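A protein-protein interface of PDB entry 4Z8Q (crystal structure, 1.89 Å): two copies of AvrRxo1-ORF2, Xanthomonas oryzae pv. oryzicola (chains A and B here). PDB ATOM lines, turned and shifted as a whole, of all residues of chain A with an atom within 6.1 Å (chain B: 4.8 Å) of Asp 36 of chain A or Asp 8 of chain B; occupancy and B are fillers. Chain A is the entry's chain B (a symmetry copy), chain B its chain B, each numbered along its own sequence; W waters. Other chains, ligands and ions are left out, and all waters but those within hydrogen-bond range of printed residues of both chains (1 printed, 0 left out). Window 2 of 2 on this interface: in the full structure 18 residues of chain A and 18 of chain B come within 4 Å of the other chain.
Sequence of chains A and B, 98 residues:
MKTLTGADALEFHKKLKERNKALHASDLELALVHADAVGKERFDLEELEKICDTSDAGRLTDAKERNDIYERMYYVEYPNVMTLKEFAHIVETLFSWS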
ATOM      1  N   ALA A  31     -19.994  19.313 -27.535  1.00  0.00           N
ATOM      2  CA  ALA A  31     -21.104  18.514 -28.069  1.00  0.00           C
ATOM      3  C   ALA A  31     -22.123  18.173 -26.995  1.00  0.00           C
ATOM      4  O   ALA A  31     -23.318  18.157 -27.270  1.00  0.00           O
ATOM      5  CB  ALA A  31     -20.601  17.225 -28.755  1.00  0.00           C
ATOM      6  N   LEU A  32     -21.650  17.898 -25.782  1.00  0.00           N
ATOM      7  CA  LEU A  32     -22.544  17.575 -24.665  1.00  0.00           C
ATOM      8  C   LEU A  32     -23.426  18.756 -24.270  1.00  0.00           C
ATOM      9  O   LEU A  32     -24.638  18.602 -24.063  1.00  0.00           O
ATOM     10  CB  LEU A  32     -21.738  17.112 -23.453  1.00  0.00           C
ATOM     11  CG  LEU A  32     -21.191  15.697 -23.644  1.00  0.00           C
ATOM     12  CD1 LEU A  32     -20.159  15.335 -22.592  1.00  0.00           C
ATOM     13  CD2 LEU A  32     -22.362  14.721 -23.631  1.00  0.00           C
ATOM     14  N   VAL A  33     -22.813  19.929 -24.155  1.00  0.00           N
ATOM     15  CA  VAL A  33     -23.564  21.134 -23.834  1.00  0.00           C
ATOM     16  C   VAL A  33     -24.652  21.327 -24.874  1.00  0.00           C
ATOM     17  O   VAL A  33     -25.826  21.495 -24.551  1.00  0.00           O
ATOM     18  CB  VAL A  33     -22.654  22.362 -23.802  1.00  0.00           C
ATOM     19  CG1 VAL A  33     -23.503  23.636 -23.662  1.00  0.00           C
ATOM     20  CG2 VAL A  33     -21.681  22.247 -22.642  1.00  0.00           C
ATOM     21  N   HIS A  34     -24.264  21.251 -26.138  1.00  0.00           N
ATOM     22  CA  HIS A  34     -25.212  21.404 -27.215  1.00  0.00           C
ATOM     23  C   HIS A  34     -26.301  20.327 -27.186  1.00  0.00           C
ATOM     24  O   HIS A  34     -27.480  20.613 -27.433  1.00  0.00           O
ATOM     25  CB  HIS A  34     -24.470  21.388 -28.548  1.00  0.00           C
ATOM     26  CG  HIS A  34     -25.359  21.592 -29.730  1.00  0.00           C
ATOM     27  ND1 HIS A  34     -25.527  22.822 -30.330  1.00  0.00           N
ATOM     28  CD2 HIS A  34     -26.136  20.723 -30.423  1.00  0.00           C
ATOM     29  CE1 HIS A  34     -26.378  22.701 -31.334  1.00  0.00           C
ATOM     30  NE2 HIS A  34     -26.751  21.435 -31.420  1.00  0.00           N
ATOM     31  N   ALA A  35     -25.913  19.090 -26.891  1.00  0.00           N
ATOM     32  CA  ALA A  35     -26.885  17.999 -26.831  1.00  0.00           C
ATOM     33  C   ALA A  35     -27.953  18.246 -25.754  1.00  0.00           C
ATOM     34  O   ALA A  35     -29.140  18.045 -26.002  1.00  0.00           O
ATOM     35  CB  ALA A  35     -26.189  16.680 -26.593  1.00  0.00           C
ATOM     36  N   ASP A  36     -27.527  18.666 -24.564  1.00  0.00           N
ATOM     37  CA  ASP A  36     -28.466  18.993 -23.485  1.00  0.00           C
ATOM     38  C   ASP A  36     -29.425  20.117 -23.881  1.00  0.00           C
ATOM     39  O   ASP A  36     -30.596  20.114 -23.497  1.00  0.00           O
ATOM     40  CB  ASP A  36     -27.709  19.384 -22.214  1.00  0.00           C
ATOM     41  CG  ASP A  36     -28.623  19.966 -21.133  1.00  0.00           C
ATOM     42  OD1 ASP A  36     -28.935  21.182 -21.193  1.00  0.00           O
ATOM     43  OD2 ASP A  36     -29.014  19.210 -20.209  1.00  0.00           O
ATOM     44  N   ALA A  37     -28.928  21.082 -24.647  1.00  0.00           N
ATOM     45  CA  ALA A  37     -29.732  22.241 -25.016  1.00  0.00           C
ATOM     46  C   ALA A  37     -30.835  21.898 -26.015  1.00  0.00           C
ATOM     47  O   ALA A  37     -31.879  22.555 -26.045  1.00  0.00           O
ATOM     48  CB  ALA A  37     -28.844  23.346 -25.569  1.00  0.00           C
ATOM     49  N   VAL A  38     -30.598  20.882 -26.839  1.00  0.00           N
ATOM     50  CA  VAL A  38     -31.558  20.523 -27.879  1.00  0.00           C
ATOM     51  C   VAL A  38     -32.372  19.287 -27.475  1.00  0.00           C
ATOM     52  O   VAL A  38     -33.202  18.800 -28.244  1.00  0.00           O
ATOM     53  CB  VAL A  38     -30.874  20.310 -29.263  1.00  0.00           C
ATOM     54  CG1 VAL A  38     -30.113  21.552 -29.676  1.00  0.00           C
ATOM     55  CG2 VAL A  38     -29.927  19.113 -29.228  1.00  0.00           C
ATOM     56  N   GLY A  39     -32.130  18.778 -26.273  1.00  0.00           N
ATOM     57  CA  GLY A  39     -32.867  17.622 -25.790  1.00  0.00           C
ATOM     58  C   GLY A  39     -32.543  16.310 -26.490  1.00  0.00           C
ATOM     59  O   GLY A  39     -33.417  15.458 -26.660  1.00  0.00           O
ATOM     60  N   LYS A  40     -31.285  16.135 -26.885  1.00  0.00           N
ATOM     61  CA  LYS A  40     -30.842  14.883 -27.486  1.00  0.00           C
ATOM     62  C   LYS A  40     -30.783  13.823 -26.403  1.00  0.00           C
ATOM     63  O   LYS A  40     -30.321  14.088 -25.286  1.00  0.00           O
ATOM     64  CB  LYS A  40     -29.468  15.084 -28.140  1.00  0.00           C
ATOM     65  CG  LYS A  40     -28.678  13.825 -28.490  1.00  0.00           C
ATOM     66  CD  LYS A  40     -27.491  14.247 -29.373  1.00  0.00           C
ATOM     67  CE  LYS A  40     -26.529  13.102 -29.629  1.00  0.00           C
ATOM     68  NZ  LYS A  40     -26.003  13.163 -31.028  1.00  0.00           N
ATOM     69  N   LEU B   4     -28.592  28.949 -27.758  1.00  0.00           N
ATOM     70  CA  LEU B   4     -28.222  28.518 -26.406  1.00  0.00           C
ATOM     71  C   LEU B   4     -28.490  29.668 -25.438  1.00  0.00           C
ATOM     72  O   LEU B   4     -28.129  30.821 -25.713  1.00  0.00           O
ATOM     73  CB  LEU B   4     -26.746  28.103 -26.342  1.00  0.00           C
ATOM     74  CG  LEU B   4     -26.192  27.135 -27.391  1.00  0.00           C
ATOM     75  CD1 LEU B   4     -24.737  26.826 -27.090  1.00  0.00           C
ATOM     76  CD2 LEU B   4     -26.974  25.854 -27.433  1.00  0.00           C
ATOM     77  N   THR B   5     -29.114  29.360 -24.300  1.00  0.00           N
ATOM     78  CA  THR B   5     -29.472  30.373 -23.311  1.00  0.00           C
ATOM     79  C   THR B   5     -29.049  29.932 -21.917  1.00  0.00           C
ATOM     80  O   THR B   5     -28.654  28.772 -21.710  1.00  0.00           O
ATOM     81  CB  THR B   5     -31.007  30.617 -23.260  1.00  0.00           C
ATOM     82  OG1 THR B   5     -31.640  29.461 -22.700  1.00  0.00           O
ATOM     83  CG2 THR B   5     -31.583  30.867 -24.654  1.00  0.00           C
ATOM     84  N   GLY B   6     -29.134  30.856 -20.965  1.00  0.00           N
ATOM     85  CA  GLY B   6     -28.907  30.544 -19.555  1.00  0.00           C
ATOM     86  C   GLY B   6     -27.659  29.727 -19.268  1.00  0.00           C
ATOM     87  O   GLY B   6     -26.566  30.042 -19.755  1.00  0.00           O
ATOM     88  N   ALA B   7     -27.822  28.674 -18.476  1.00  0.00           N
ATOM     89  CA  ALA B   7     -26.712  27.847 -18.047  1.00  0.00           C
ATOM     90  C   ALA B   7     -25.986  27.223 -19.234  1.00  0.00           C
ATOM     91  O   ALA B   7     -24.760  27.139 -19.232  1.00  0.00           O
ATOM     92  CB  ALA B   7     -27.195  26.762 -17.054  1.00  0.00           C
ATOM     93  N   ASP B   8     -26.724  26.793 -20.252  1.00  0.00           N
ATOM     94  CA  ASP B   8     -26.071  26.151 -21.391  1.00  0.00           C
ATOM     95  C   ASP B   8     -25.192  27.131 -22.160  1.00  0.00           C
ATOM     96  O   ASP B   8     -24.083  26.790 -22.568  1.00  0.00           O
ATOM     97  CB  ASP B   8     -27.087  25.491 -22.328  1.00  0.00           C
ATOM     98  CG  ASP B   8     -27.629  24.173 -21.778  1.00  0.00           C
ATOM     99  OD1 ASP B   8     -27.133  23.699 -20.735  1.00  0.00           O
ATOM    100  OD2 ASP B   8     -28.546  23.606 -22.402  1.00  0.00           O
ATOM    101  N   ALA B   9     -25.687  28.350 -22.366  1.00  0.00           N
ATOM    102  CA  ALA B   9     -24.906  29.357 -23.071  1.00  0.00           C
ATOM    103  C   ALA B   9     -23.623  29.613 -22.297  1.00  0.00           C
ATOM    104  O   ALA B   9     -22.532  29.623 -22.861  1.00  0.00           O
ATOM    105  CB  ALA B   9     -25.707  30.657 -23.226  1.00  0.00           C
ATOM    106  N   LEU B  10     -23.751  29.835 -20.996  1.00  0.00           N
ATOM    107  CA  LEU B  10     -22.573  30.114 -20.173  1.00  0.00           C
ATOM    108  C   LEU B  10     -21.581  28.967 -20.196  1.00  0.00           C
ATOM    109  O   LEU B  10     -20.387  29.194 -20.250  1.00  0.00           O
ATOM    110  CB  LEU B  10     -22.972  30.425 -18.721  1.00  0.00           C
ATOM    111  CG  LEU B  10     -23.556  31.805 -18.447  1.00  0.00           C
ATOM    112  CD1 LEU B  10     -24.084  31.884 -16.996  1.00  0.00           C
ATOM    113  CD2 LEU B  10     -22.513  32.873 -18.686  1.00  0.00           C
ATOM    114  N   GLU B  11     -22.075  27.734 -20.158  1.00  0.00           N
ATOM    115  CA  GLU B  11     -21.177  26.583 -20.169  1.00  0.00           C
ATOM    116  C   GLU B  11     -20.512  26.400 -21.531  1.00  0.00           C
ATOM    117  O   GLU B  11     -19.346  26.016 -21.599  1.00  0.00           O
ATOM    118  CB  GLU B  11     -21.908  25.301 -19.744  1.00  0.00           C
ATOM    119  CG  GLU B  11     -20.988  24.110 -19.477  1.00  0.00           C
ATOM    120  CD  GLU B  11     -20.127  24.281 -18.225  1.00  0.00           C
ATOM    121  OE1 GLU B  11     -20.348  25.241 -17.455  1.00  0.00           O
ATOM    122  OE2 GLU B  11     -19.223  23.440 -18.007  1.00  0.00           O
ATOM    123  N   PHE B  12     -21.239  26.669 -22.613  1.00  0.00           N
ATOM    124  CA  PHE B  12     -20.634  26.589 -23.951  1.00  0.00           C
ATOM    125  C   PHE B  12     -19.504  27.588 -24.051  1.00  0.00           C
ATOM    126  O   PHE B  12     -18.445  27.289 -24.600  1.00  0.00           O
ATOM    127  CB  PHE B  12     -21.653  26.901 -25.040  1.00  0.00           C
ATOM    128  CG  PHE B  12     -21.211  26.474 -26.430  1.00  0.00           C
ATOM    129  CD1 PHE B  12     -21.377  25.158 -26.844  1.00  0.00           C
ATOM    130  CD2 PHE B  12     -20.657  27.385 -27.317  1.00  0.00           C
ATOM    131  CE1 PHE B  12     -20.991  24.752 -28.125  1.00  0.00           C
ATOM    132  CE2 PHE B  12     -20.255  26.979 -28.600  1.00  0.00           C
ATOM    133  CZ  PHE B  12     -20.435  25.662 -28.994  1.00  0.00           C
HETATM  134  O   HOH W   1     -29.589  23.365 -18.953  1.00  0.00           O
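Among the printed residues, merely in contact across the chains: Val 33 of chain A with Asp 8 of chain B (3.4 Å), Val 33 of chain A with Glu 11 of chain B (3.7 Å), Val 33 of chain A with Phe 12 of chain B (3.9 Å) and Ala 37 of chain A with Leu 4 of chain B (3.6 Å).
Printed residues of chain B within 4 Å of Val 33 of chain A: Asp 8, Glu 11 and Phe 12. Printed residues of chain B within 4 Å of Ala 37 of chain A: Leu 4 (3.6 Å) and Asp 8 (3.2 Å). Of the printed residues of chain A, Leu 4 of chain B touches Ala 37. Of the printed residues of chain A, Glu 11 of chain B touches Val 33 (3.7 Å). Printed residues of chain A within 4 Å of Phe 12 of chain B: Val 33. The nearest residue of chain A that does not touch Asp 8 of chain B is Val 38 of chain A (5.6 Å).
Hydrophobic or aromatic side chains of chain A within 4 Å of the printed part of chain B: Val 33 and Ala 37. Of the 9 printed residues of chain B, 4 touch a printed residue of chain A. Printed residues of chain B that touch a printed residue of chain A: Leu 4, Asp 8, Glu 11 and Phe 12. Among the printed residues, no Asp or Glu carboxylate lies within 4 Å of a Lys or Arg side-chain nitrogen of the other chain.
The side-chain carboxylate (OD2) of Asp 8 of chain B sits close to the side-chain carboxylate (OD1) of Asp 36 of chain A (2.7 Å). The backbone NH (N) of Ala 37 of chain A lies close to the side-chain carboxylate (OD2) of Asp 8 of chain B, 3.4 Å away.
No position is printed for both chains. Of the 6 pairs that touch across the chains among the printed residues, none has its exchanged pair printed and touching as well.
Water W1 lies within hydrogen-bond range of OD1 of Asp 8 of chain B (3.1 Å) and OD1 of Asp 36 of chain A (3.2 Å).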
